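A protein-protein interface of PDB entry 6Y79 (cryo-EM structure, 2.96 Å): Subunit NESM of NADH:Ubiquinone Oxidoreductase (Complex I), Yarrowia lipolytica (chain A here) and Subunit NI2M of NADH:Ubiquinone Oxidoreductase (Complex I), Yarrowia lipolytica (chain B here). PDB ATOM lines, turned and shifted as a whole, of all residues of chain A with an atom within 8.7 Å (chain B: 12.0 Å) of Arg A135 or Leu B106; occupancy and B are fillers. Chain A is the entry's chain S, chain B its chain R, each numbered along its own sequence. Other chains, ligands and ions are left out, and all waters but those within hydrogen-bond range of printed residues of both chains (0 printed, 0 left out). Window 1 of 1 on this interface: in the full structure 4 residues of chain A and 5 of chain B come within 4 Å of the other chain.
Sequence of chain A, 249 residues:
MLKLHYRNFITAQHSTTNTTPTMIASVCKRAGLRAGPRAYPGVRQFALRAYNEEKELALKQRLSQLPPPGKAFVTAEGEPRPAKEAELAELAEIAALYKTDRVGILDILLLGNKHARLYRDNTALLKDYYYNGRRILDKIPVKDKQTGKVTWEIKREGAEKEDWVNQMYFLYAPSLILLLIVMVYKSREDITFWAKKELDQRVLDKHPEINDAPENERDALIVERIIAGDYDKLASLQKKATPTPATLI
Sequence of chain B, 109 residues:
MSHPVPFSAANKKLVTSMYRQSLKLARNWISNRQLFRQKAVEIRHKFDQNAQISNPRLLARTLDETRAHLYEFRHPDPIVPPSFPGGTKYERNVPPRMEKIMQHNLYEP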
ATOM      1  N   PRO A  69      27.950  25.541  24.408  1.00  0.00           N
ATOM      2  CA  PRO A  69      26.522  25.884  24.387  1.00  0.00           C
ATOM      3  C   PRO A  69      26.216  27.217  25.030  1.00  0.00           C
ATOM      4  O   PRO A  69      25.121  27.752  24.823  1.00  0.00           O
ATOM      5  CB  PRO A  69      25.878  24.722  25.154  1.00  0.00           C
ATOM      6  CG  PRO A  69      26.922  23.636  25.156  1.00  0.00           C
ATOM      7  CD  PRO A  69      28.207  24.360  25.250  1.00  0.00           C
ATOM      8  N   PHE A  73      24.146  29.958  20.844  1.00  0.00           N
ATOM      9  CA  PHE A  73      22.891  30.617  20.539  1.00  0.00           C
ATOM     10  C   PHE A  73      22.802  32.047  21.055  1.00  0.00           C
ATOM     11  O   PHE A  73      21.756  32.675  20.869  1.00  0.00           O
ATOM     12  CB  PHE A  73      21.718  29.818  21.110  1.00  0.00           C
ATOM     13  CG  PHE A  73      21.573  28.457  20.524  1.00  0.00           C
ATOM     14  CD1 PHE A  73      20.852  28.268  19.363  1.00  0.00           C
ATOM     15  CD2 PHE A  73      22.148  27.363  21.143  1.00  0.00           C
ATOM     16  CE1 PHE A  73      20.711  27.009  18.828  1.00  0.00           C
ATOM     17  CE2 PHE A  73      22.012  26.106  20.614  1.00  0.00           C
ATOM     18  CZ  PHE A  73      21.295  25.928  19.456  1.00  0.00           C
ATOM     19  N   ALA A  76      22.077  37.132  19.639  1.00  0.00           N
ATOM     20  CA  ALA A  76      20.781  37.782  19.900  1.00  0.00           C
ATOM     21  C   ALA A  76      19.636  36.798  20.143  1.00  0.00           C
ATOM     22  O   ALA A  76      19.714  35.941  21.022  1.00  0.00           O
ATOM     23  CB  ALA A  76      20.421  38.739  18.760  1.00  0.00           C
ATOM     24  N   LYS A 127      21.889  16.989  24.690  1.00  0.00           N
ATOM     25  CA  LYS A 127      20.837  17.541  25.535  1.00  0.00           C
ATOM     26  C   LYS A 127      21.060  19.025  25.781  1.00  0.00           C
ATOM     27  O   LYS A 127      20.108  19.821  25.781  1.00  0.00           O
ATOM     28  CB  LYS A 127      20.804  16.761  26.848  1.00  0.00           C
ATOM     29  CG  LYS A 127      19.934  17.337  27.933  1.00  0.00           C
ATOM     30  CD  LYS A 127      20.039  16.526  29.209  1.00  0.00           C
ATOM     31  CE  LYS A 127      18.942  16.903  30.186  1.00  0.00           C
ATOM     32  NZ  LYS A 127      18.993  16.076  31.418  1.00  0.00           N
ATOM     33  N   ASP A 128      22.326  19.414  25.952  1.00  0.00           N
ATOM     34  CA  ASP A 128      22.672  20.821  26.110  1.00  0.00           C
ATOM     35  C   ASP A 128      22.319  21.634  24.870  1.00  0.00           C
ATOM     36  O   ASP A 128      21.694  22.706  24.974  1.00  0.00           O
ATOM     37  CB  ASP A 128      24.158  20.909  26.432  1.00  0.00           C
ATOM     38  CG  ASP A 128      24.501  22.109  27.288  1.00  0.00           C
ATOM     39  OD1 ASP A 128      23.636  22.990  27.412  1.00  0.00           O
ATOM     40  OD2 ASP A 128      25.633  22.178  27.798  1.00  0.00           O
ATOM     41  N   TYR A 129      22.658  21.105  23.689  1.00  0.00           N
ATOM     42  CA  TYR A 129      22.344  21.789  22.440  1.00  0.00           C
ATOM     43  C   TYR A 129      20.847  21.816  22.154  1.00  0.00           C
ATOM     44  O   TYR A 129      20.369  22.714  21.451  1.00  0.00           O
ATOM     45  CB  TYR A 129      23.073  21.120  21.280  1.00  0.00           C
ATOM     46  CG  TYR A 129      24.554  21.377  21.244  1.00  0.00           C
ATOM     47  CD1 TYR A 129      25.090  22.542  21.795  1.00  0.00           C
ATOM     48  CD2 TYR A 129      25.424  20.458  20.674  1.00  0.00           C
ATOM     49  CE1 TYR A 129      26.445  22.781  21.758  1.00  0.00           C
ATOM     50  CE2 TYR A 129      26.775  20.693  20.645  1.00  0.00           C
ATOM     51  CZ  TYR A 129      27.281  21.841  21.184  1.00  0.00           C
ATOM     52  OH  TYR A 129      28.636  22.082  21.160  1.00  0.00           O
ATOM     53  N   TYR A 130      20.095  20.847  22.670  1.00  0.00           N
ATOM     54  CA  TYR A 130      18.650  20.880  22.492  1.00  0.00           C
ATOM     55  C   TYR A 130      18.026  21.959  23.357  1.00  0.00           C
ATOM     56  O   TYR A 130      17.286  22.818  22.860  1.00  0.00           O
ATOM     57  CB  TYR A 130      18.041  19.518  22.820  1.00  0.00           C
ATOM     58  CG  TYR A 130      16.534  19.458  22.650  1.00  0.00           C
ATOM     59  CD1 TYR A 130      15.963  19.325  21.394  1.00  0.00           C
ATOM     60  CD2 TYR A 130      15.687  19.523  23.746  1.00  0.00           C
ATOM     61  CE1 TYR A 130      14.592  19.266  21.231  1.00  0.00           C
ATOM     62  CE2 TYR A 130      14.314  19.466  23.597  1.00  0.00           C
ATOM     63  CZ  TYR A 130      13.772  19.339  22.339  1.00  0.00           C
ATOM     64  OH  TYR A 130      12.404  19.282  22.192  1.00  0.00           O
ATOM     65  N   TYR A 131      18.324  21.943  24.658  1.00  0.00           N
ATOM     66  CA  TYR A 131      17.574  22.801  25.566  1.00  0.00           C
ATOM     67  C   TYR A 131      18.024  24.256  25.511  1.00  0.00           C
ATOM     68  O   TYR A 131      17.188  25.145  25.700  1.00  0.00           O
ATOM     69  CB  TYR A 131      17.637  22.251  26.990  1.00  0.00           C
ATOM     70  CG  TYR A 131      16.790  21.009  27.168  1.00  0.00           C
ATOM     71  CD1 TYR A 131      15.407  21.080  27.222  1.00  0.00           C
ATOM     72  CD2 TYR A 131      17.377  19.763  27.262  1.00  0.00           C
ATOM     73  CE1 TYR A 131      14.643  19.940  27.371  1.00  0.00           C
ATOM     74  CE2 TYR A 131      16.627  18.626  27.406  1.00  0.00           C
ATOM     75  CZ  TYR A 131      15.263  18.717  27.464  1.00  0.00           C
ATOM     76  OH  TYR A 131      14.524  17.569  27.614  1.00  0.00           O
ATOM     77  N   ASN A 132      19.296  24.549  25.207  1.00  0.00           N
ATOM     78  CA  ASN A 132      19.671  25.958  25.087  1.00  0.00           C
ATOM     79  C   ASN A 132      19.107  26.585  23.821  1.00  0.00           C
ATOM     80  O   ASN A 132      18.748  27.771  23.807  1.00  0.00           O
ATOM     81  CB  ASN A 132      21.182  26.115  25.140  1.00  0.00           C
ATOM     82  CG  ASN A 132      21.674  26.329  26.538  1.00  0.00           C
ATOM     83  OD1 ASN A 132      22.232  25.427  27.152  1.00  0.00           O
ATOM     84  ND2 ASN A 132      21.466  27.532  27.060  1.00  0.00           N
ATOM     85  N   GLY A 133      19.007  25.799  22.752  1.00  0.00           N
ATOM     86  CA  GLY A 133      18.331  26.274  21.565  1.00  0.00           C
ATOM     87  C   GLY A 133      16.845  26.445  21.771  1.00  0.00           C
ATOM     88  O   GLY A 133      16.249  27.374  21.226  1.00  0.00           O
ATOM     89  N   ARG A 134      16.230  25.567  22.564  1.00  0.00           N
ATOM     90  CA  ARG A 134      14.822  25.740  22.907  1.00  0.00           C
ATOM     91  C   ARG A 134      14.596  26.985  23.757  1.00  0.00           C
ATOM     92  O   ARG A 134      13.550  27.630  23.648  1.00  0.00           O
ATOM     93  CB  ARG A 134      14.315  24.497  23.634  1.00  0.00           C
ATOM     94  CG  ARG A 134      12.829  24.465  23.851  1.00  0.00           C
ATOM     95  CD  ARG A 134      12.420  23.259  24.660  1.00  0.00           C
ATOM     96  NE  ARG A 134      10.999  23.314  24.969  1.00  0.00           N
ATOM     97  CZ  ARG A 134      10.312  22.323  25.522  1.00  0.00           C
ATOM     98  NH1 ARG A 134      10.915  21.185  25.825  1.00  0.00           N
ATOM     99  NH2 ARG A 134       9.019  22.472  25.761  1.00  0.00           N
ATOM    100  N   ARG A 135      15.568  27.347  24.593  1.00  0.00           N
ATOM    101  CA  ARG A 135      15.415  28.547  25.408  1.00  0.00           C
ATOM    102  C   ARG A 135      15.599  29.825  24.604  1.00  0.00           C
ATOM    103  O   ARG A 135      14.810  30.764  24.750  1.00  0.00           O
ATOM    104  CB  ARG A 135      16.389  28.522  26.576  1.00  0.00           C
ATOM    105  CG  ARG A 135      15.951  27.621  27.691  1.00  0.00           C
ATOM    106  CD  ARG A 135      14.564  27.981  28.225  1.00  0.00           C
ATOM    107  NE  ARG A 135      13.542  27.059  27.739  1.00  0.00           N
ATOM    108  CZ  ARG A 135      12.260  27.134  28.056  1.00  0.00           C
ATOM    109  NH1 ARG A 135      11.396  26.256  27.564  1.00  0.00           N
ATOM    110  NH2 ARG A 135      11.845  28.077  28.877  1.00  0.00           N
ATOM    111  N   ILE A 136      16.637  29.892  23.770  1.00  0.00           N
ATOM    112  CA  ILE A 136      16.871  31.108  22.995  1.00  0.00           C
ATOM    113  C   ILE A 136      15.858  31.227  21.861  1.00  0.00           C
ATOM    114  O   ILE A 136      15.367  32.320  21.555  1.00  0.00           O
ATOM    115  CB  ILE A 136      18.320  31.133  22.482  1.00  0.00           C
ATOM    116  CG1 ILE A 136      19.290  31.055  23.662  1.00  0.00           C
ATOM    117  CG2 ILE A 136      18.591  32.384  21.677  1.00  0.00           C
ATOM    118  CD1 ILE A 136      19.071  32.124  24.707  1.00  0.00           C
ATOM    119  N   LEU A 137      15.501  30.115  21.241  1.00  0.00           N
ATOM    120  CA  LEU A 137      14.585  30.170  20.110  1.00  0.00           C
ATOM    121  C   LEU A 137      13.204  29.609  20.477  1.00  0.00           C
ATOM    122  O   LEU A 137      12.333  30.329  20.971  1.00  0.00           O
ATOM    123  CB  LEU A 137      15.173  29.411  18.913  1.00  0.00           C
ATOM    124  CG  LEU A 137      16.272  30.039  18.036  1.00  0.00           C
ATOM    125  CD1 LEU A 137      17.656  30.091  18.676  1.00  0.00           C
ATOM    126  CD2 LEU A 137      16.381  29.289  16.756  1.00  0.00           C
ATOM    127  N   GLU A 153      14.054  23.394  16.474  1.00  0.00           N
ATOM    128  CA  GLU A 153      13.953  24.578  17.318  1.00  0.00           C
ATOM    129  C   GLU A 153      12.922  25.597  16.818  1.00  0.00           C
ATOM    130  O   GLU A 153      12.117  26.096  17.614  1.00  0.00           O
ATOM    131  CB  GLU A 153      15.329  25.238  17.420  1.00  0.00           C
ATOM    132  CG  GLU A 153      16.442  24.287  17.819  1.00  0.00           C
ATOM    133  CD  GLU A 153      17.807  24.908  17.648  1.00  0.00           C
ATOM    134  OE1 GLU A 153      17.915  25.899  16.898  1.00  0.00           O
ATOM    135  OE2 GLU A 153      18.763  24.417  18.280  1.00  0.00           O
ATOM    136  N   GLU A 162       7.440  15.437  28.569  1.00  0.00           N
ATOM    137  CA  GLU A 162       8.595  15.574  29.441  1.00  0.00           C
ATOM    138  C   GLU A 162       8.890  14.244  30.136  1.00  0.00           C
ATOM    139  O   GLU A 162       8.085  13.312  30.120  1.00  0.00           O
ATOM    140  CB  GLU A 162       8.374  16.716  30.430  1.00  0.00           C
ATOM    141  CG  GLU A 162       8.428  18.055  29.730  1.00  0.00           C
ATOM    142  CD  GLU A 162       8.354  19.213  30.683  1.00  0.00           C
ATOM    143  OE1 GLU A 162       8.211  18.958  31.893  1.00  0.00           O
ATOM    144  OE2 GLU A 162       8.427  20.373  30.224  1.00  0.00           O
ATOM    145  N   LYS B 100       6.683  40.827  28.499  1.00  0.00           N
ATOM    146  CA  LYS B 100       6.919  39.484  28.013  1.00  0.00           C
ATOM    147  C   LYS B 100       7.458  38.624  29.151  1.00  0.00           C
ATOM    148  O   LYS B 100       7.938  39.124  30.168  1.00  0.00           O
ATOM    149  CB  LYS B 100       7.882  39.492  26.824  1.00  0.00           C
ATOM    150  CG  LYS B 100       7.208  39.633  25.457  1.00  0.00           C
ATOM    151  CD  LYS B 100       6.804  41.072  25.165  1.00  0.00           C
ATOM    152  CE  LYS B 100       8.020  41.963  24.997  1.00  0.00           C
ATOM    153  NZ  LYS B 100       7.639  43.390  24.812  1.00  0.00           N
ATOM    154  N   ILE B 101       7.371  37.314  28.967  1.00  0.00           N
ATOM    155  CA  ILE B 101       7.630  36.371  30.046  1.00  0.00           C
ATOM    156  C   ILE B 101       9.131  36.216  30.248  1.00  0.00           C
ATOM    157  O   ILE B 101       9.855  35.816  29.332  1.00  0.00           O
ATOM    158  CB  ILE B 101       6.978  35.019  29.749  1.00  0.00           C
ATOM    159  CG1 ILE B 101       5.463  35.158  29.708  1.00  0.00           C
ATOM    160  CG2 ILE B 101       7.374  34.016  30.780  1.00  0.00           C
ATOM    161  CD1 ILE B 101       4.768  33.923  29.219  1.00  0.00           C
ATOM    162  N   MET B 102       9.600  36.535  31.450  1.00  0.00           N
ATOM    163  CA  MET B 102      10.960  36.213  31.855  1.00  0.00           C
ATOM    164  C   MET B 102      11.023  34.743  32.233  1.00  0.00           C
ATOM    165  O   MET B 102      10.077  34.201  32.805  1.00  0.00           O
ATOM    166  CB  MET B 102      11.376  37.087  33.035  1.00  0.00           C
ATOM    167  CG  MET B 102      12.794  36.921  33.506  1.00  0.00           C
ATOM    168  SD  MET B 102      13.926  37.774  32.420  1.00  0.00           S
ATOM    169  CE  MET B 102      13.383  39.455  32.675  1.00  0.00           C
ATOM    170  N   GLN B 103      12.122  34.083  31.903  1.00  0.00           N
ATOM    171  CA  GLN B 103      12.209  32.650  32.121  1.00  0.00           C
ATOM    172  C   GLN B 103      13.312  32.314  33.112  1.00  0.00           C
ATOM    173  O   GLN B 103      14.359  32.964  33.155  1.00  0.00           O
ATOM    174  CB  GLN B 103      12.396  31.919  30.803  1.00  0.00           C
ATOM    175  CG  GLN B 103      11.113  31.924  30.014  1.00  0.00           C
ATOM    176  CD  GLN B 103      11.200  31.156  28.737  1.00  0.00           C
ATOM    177  OE1 GLN B 103      12.240  30.583  28.415  1.00  0.00           O
ATOM    178  NE2 GLN B 103      10.103  31.122  27.994  1.00  0.00           N
ATOM    179  N   HIS B 104      13.049  31.292  33.918  1.00  0.00           N
ATOM    180  CA  HIS B 104      13.865  30.955  35.069  1.00  0.00           C
ATOM    181  C   HIS B 104      14.474  29.565  34.991  1.00  0.00           C
ATOM    182  O   HIS B 104      15.334  29.241  35.814  1.00  0.00           O
ATOM    183  CB  HIS B 104      13.024  31.051  36.352  1.00  0.00           C
ATOM    184  CG  HIS B 104      11.922  30.042  36.409  1.00  0.00           C
ATOM    185  ND1 HIS B 104      10.741  30.194  35.720  1.00  0.00           N
ATOM    186  CD2 HIS B 104      11.839  28.848  37.038  1.00  0.00           C
ATOM    187  CE1 HIS B 104       9.973  29.142  35.933  1.00  0.00           C
ATOM    188  NE2 HIS B 104      10.617  28.309  36.727  1.00  0.00           N
ATOM    189  N   ASN B 105      14.069  28.743  34.035  1.00  0.00           N
ATOM    190  CA  ASN B 105      14.523  27.366  33.961  1.00  0.00           C
ATOM    191  C   ASN B 105      14.921  27.033  32.532  1.00  0.00           C
ATOM    192  O   ASN B 105      14.284  27.482  31.577  1.00  0.00           O
ATOM    193  CB  ASN B 105      13.429  26.417  34.456  1.00  0.00           C
ATOM    194  CG  ASN B 105      13.941  25.028  34.722  1.00  0.00           C
ATOM    195  OD1 ASN B 105      15.148  24.788  34.753  1.00  0.00           O
ATOM    196  ND2 ASN B 105      13.026  24.102  34.933  1.00  0.00           N
ATOM    197  N   LEU B 106      15.985  26.242  32.399  1.00  0.00           N
ATOM    198  CA  LEU B 106      16.466  25.848  31.084  1.00  0.00           C
ATOM    199  C   LEU B 106      15.543  24.838  30.420  1.00  0.00           C
ATOM    200  O   LEU B 106      15.442  24.799  29.193  1.00  0.00           O
ATOM    201  CB  LEU B 106      17.868  25.260  31.217  1.00  0.00           C
ATOM    202  CG  LEU B 106      18.629  24.761  29.992  1.00  0.00           C
ATOM    203  CD1 LEU B 106      18.922  25.902  29.075  1.00  0.00           C
ATOM    204  CD2 LEU B 106      19.912  24.084  30.413  1.00  0.00           C
ATOM    205  N   TYR B 107      14.854  24.020  31.201  1.00  0.00           N
ATOM    206  CA  TYR B 107      14.190  22.841  30.668  1.00  0.00           C
ATOM    207  C   TYR B 107      12.685  23.006  30.570  1.00  0.00           C
ATOM    208  O   TYR B 107      12.055  22.521  29.624  1.00  0.00           O
ATOM    209  CB  TYR B 107      14.523  21.636  31.543  1.00  0.00           C
ATOM    210  CG  TYR B 107      16.000  21.357  31.638  1.00  0.00           C
ATOM    211  CD1 TYR B 107      16.642  20.597  30.673  1.00  0.00           C
ATOM    212  CD2 TYR B 107      16.759  21.857  32.690  1.00  0.00           C
ATOM    213  CE1 TYR B 107      17.988  20.344  30.751  1.00  0.00           C
ATOM    214  CE2 TYR B 107      18.109  21.608  32.771  1.00  0.00           C
ATOM    215  CZ  TYR B 107      18.716  20.851  31.802  1.00  0.00           C
ATOM    216  OH  TYR B 107      20.063  20.597  31.886  1.00  0.00           O
ATOM    217  N   GLU B 108      12.098  23.698  31.527  1.00  0.00           N
ATOM    218  CA  GLU B 108      10.666  23.762  31.735  1.00  0.00           C
ATOM    219  C   GLU B 108      10.222  25.213  31.647  1.00  0.00           C
ATOM    220  O   GLU B 108      10.982  26.109  32.018  1.00  0.00           O
ATOM    221  CB  GLU B 108      10.351  23.184  33.116  1.00  0.00           C
ATOM    222  CG  GLU B 108       9.007  23.465  33.729  1.00  0.00           C
ATOM    223  CD  GLU B 108       9.064  23.367  35.244  1.00  0.00           C
ATOM    224  OE1 GLU B 108       9.924  24.039  35.848  1.00  0.00           O
ATOM    225  OE2 GLU B 108       8.281  22.602  35.834  1.00  0.00           O
ATOM    226  N   PRO B 109       9.045  25.489  31.083  1.00  0.00           N
ATOM    227  CA  PRO B 109       8.572  26.868  31.215  1.00  0.00           C
ATOM    228  C   PRO B 109       8.184  27.186  32.647  1.00  0.00           C
ATOM    229  O   PRO B 109       9.046  27.704  33.351  1.00  0.00           O
ATOM    230  CB  PRO B 109       7.360  26.903  30.295  1.00  0.00           C
ATOM    231  CG  PRO B 109       7.603  25.845  29.301  1.00  0.00           C
ATOM    232  CD  PRO B 109       8.282  24.748  30.071  1.00  0.00           C
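OE1 of Gln B103 lies within hydrogen-bond range of NH2 of Arg A135 (2.6 Å).
The backbone carbonyl oxygen (O) of Leu B106 lies close to the guanidinium group (NE) of Arg A135, 3.3 Å away.
The side-chain amide nitrogen (ND2) of Asn B105 sits at hydrogen-bond distance from the side-chain carboxylate (OE1) of Glu B108, at 3.2 Å.
OD1 of Asn A132 sits close to OD1 of Asp A128, 2.8 Å away.
Lys A127 touches Tyr B107 (CE to CE1, 3.6 Å).
Tyr A131 touches Leu B106.
Tyr B107 touches Tyr A131.
ND2 of Asn A132 touches CD1 of Leu B106, 3.6 Å away.
Asn B105 touches Arg A135.
Arg A135 touches Glu B108.
Ala A76 touches none of the printed residues of chain B.
Of the printed residues of chain B, Lys A127 touches Tyr B107.
No residue of chain B comes within 4 Å of Asp A128.
Tyr A131 touches two residues of chain B.
Asn A132 touches one residue of chain B.
Gly A133 touches none of the printed residues of chain B.
Arg A135 touches just these residues of chain B: Gln B103 (2.6 Å), Asn B105 (3.4 Å), Leu B106 (3.2 Å) and Glu B108 (3.8 Å).
No residue of chain B comes within 4 Å of Ile A136.
No residue of chain B comes within 4 Å of Leu A137.
Printed residues of chain A within 4 Å of Gln B103: Arg A135 (2.6 Å).
Asn B105 touches one residue of chain A.
Leu B106 touches three residues of chain A.
Of chain A, only Lys A127 and Tyr A131 come within 4 Å of Tyr B107.
Of the printed residues of chain A, Glu B108 touches Arg A135 (3.8 Å).
Pro B109 touches none of the printed residues of chain A.
The nearest printed residue of chain B that does not touch Lys A127 is Leu B106 (6.3 Å).
Of the 16 printed residues of chain A, 4 touch a printed residue of chain B.
Of the 10 printed residues of chain B, 5 touch a printed residue of chain A.
Printed residues of chain B that touch a printed residue of chain A: Gln B103, Asn B105, Leu B106, Tyr B107 and Glu B108.
Hydrophobic or aromatic side chains of chain B that line the printed part of chain A: Leu B106 and Tyr B107.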
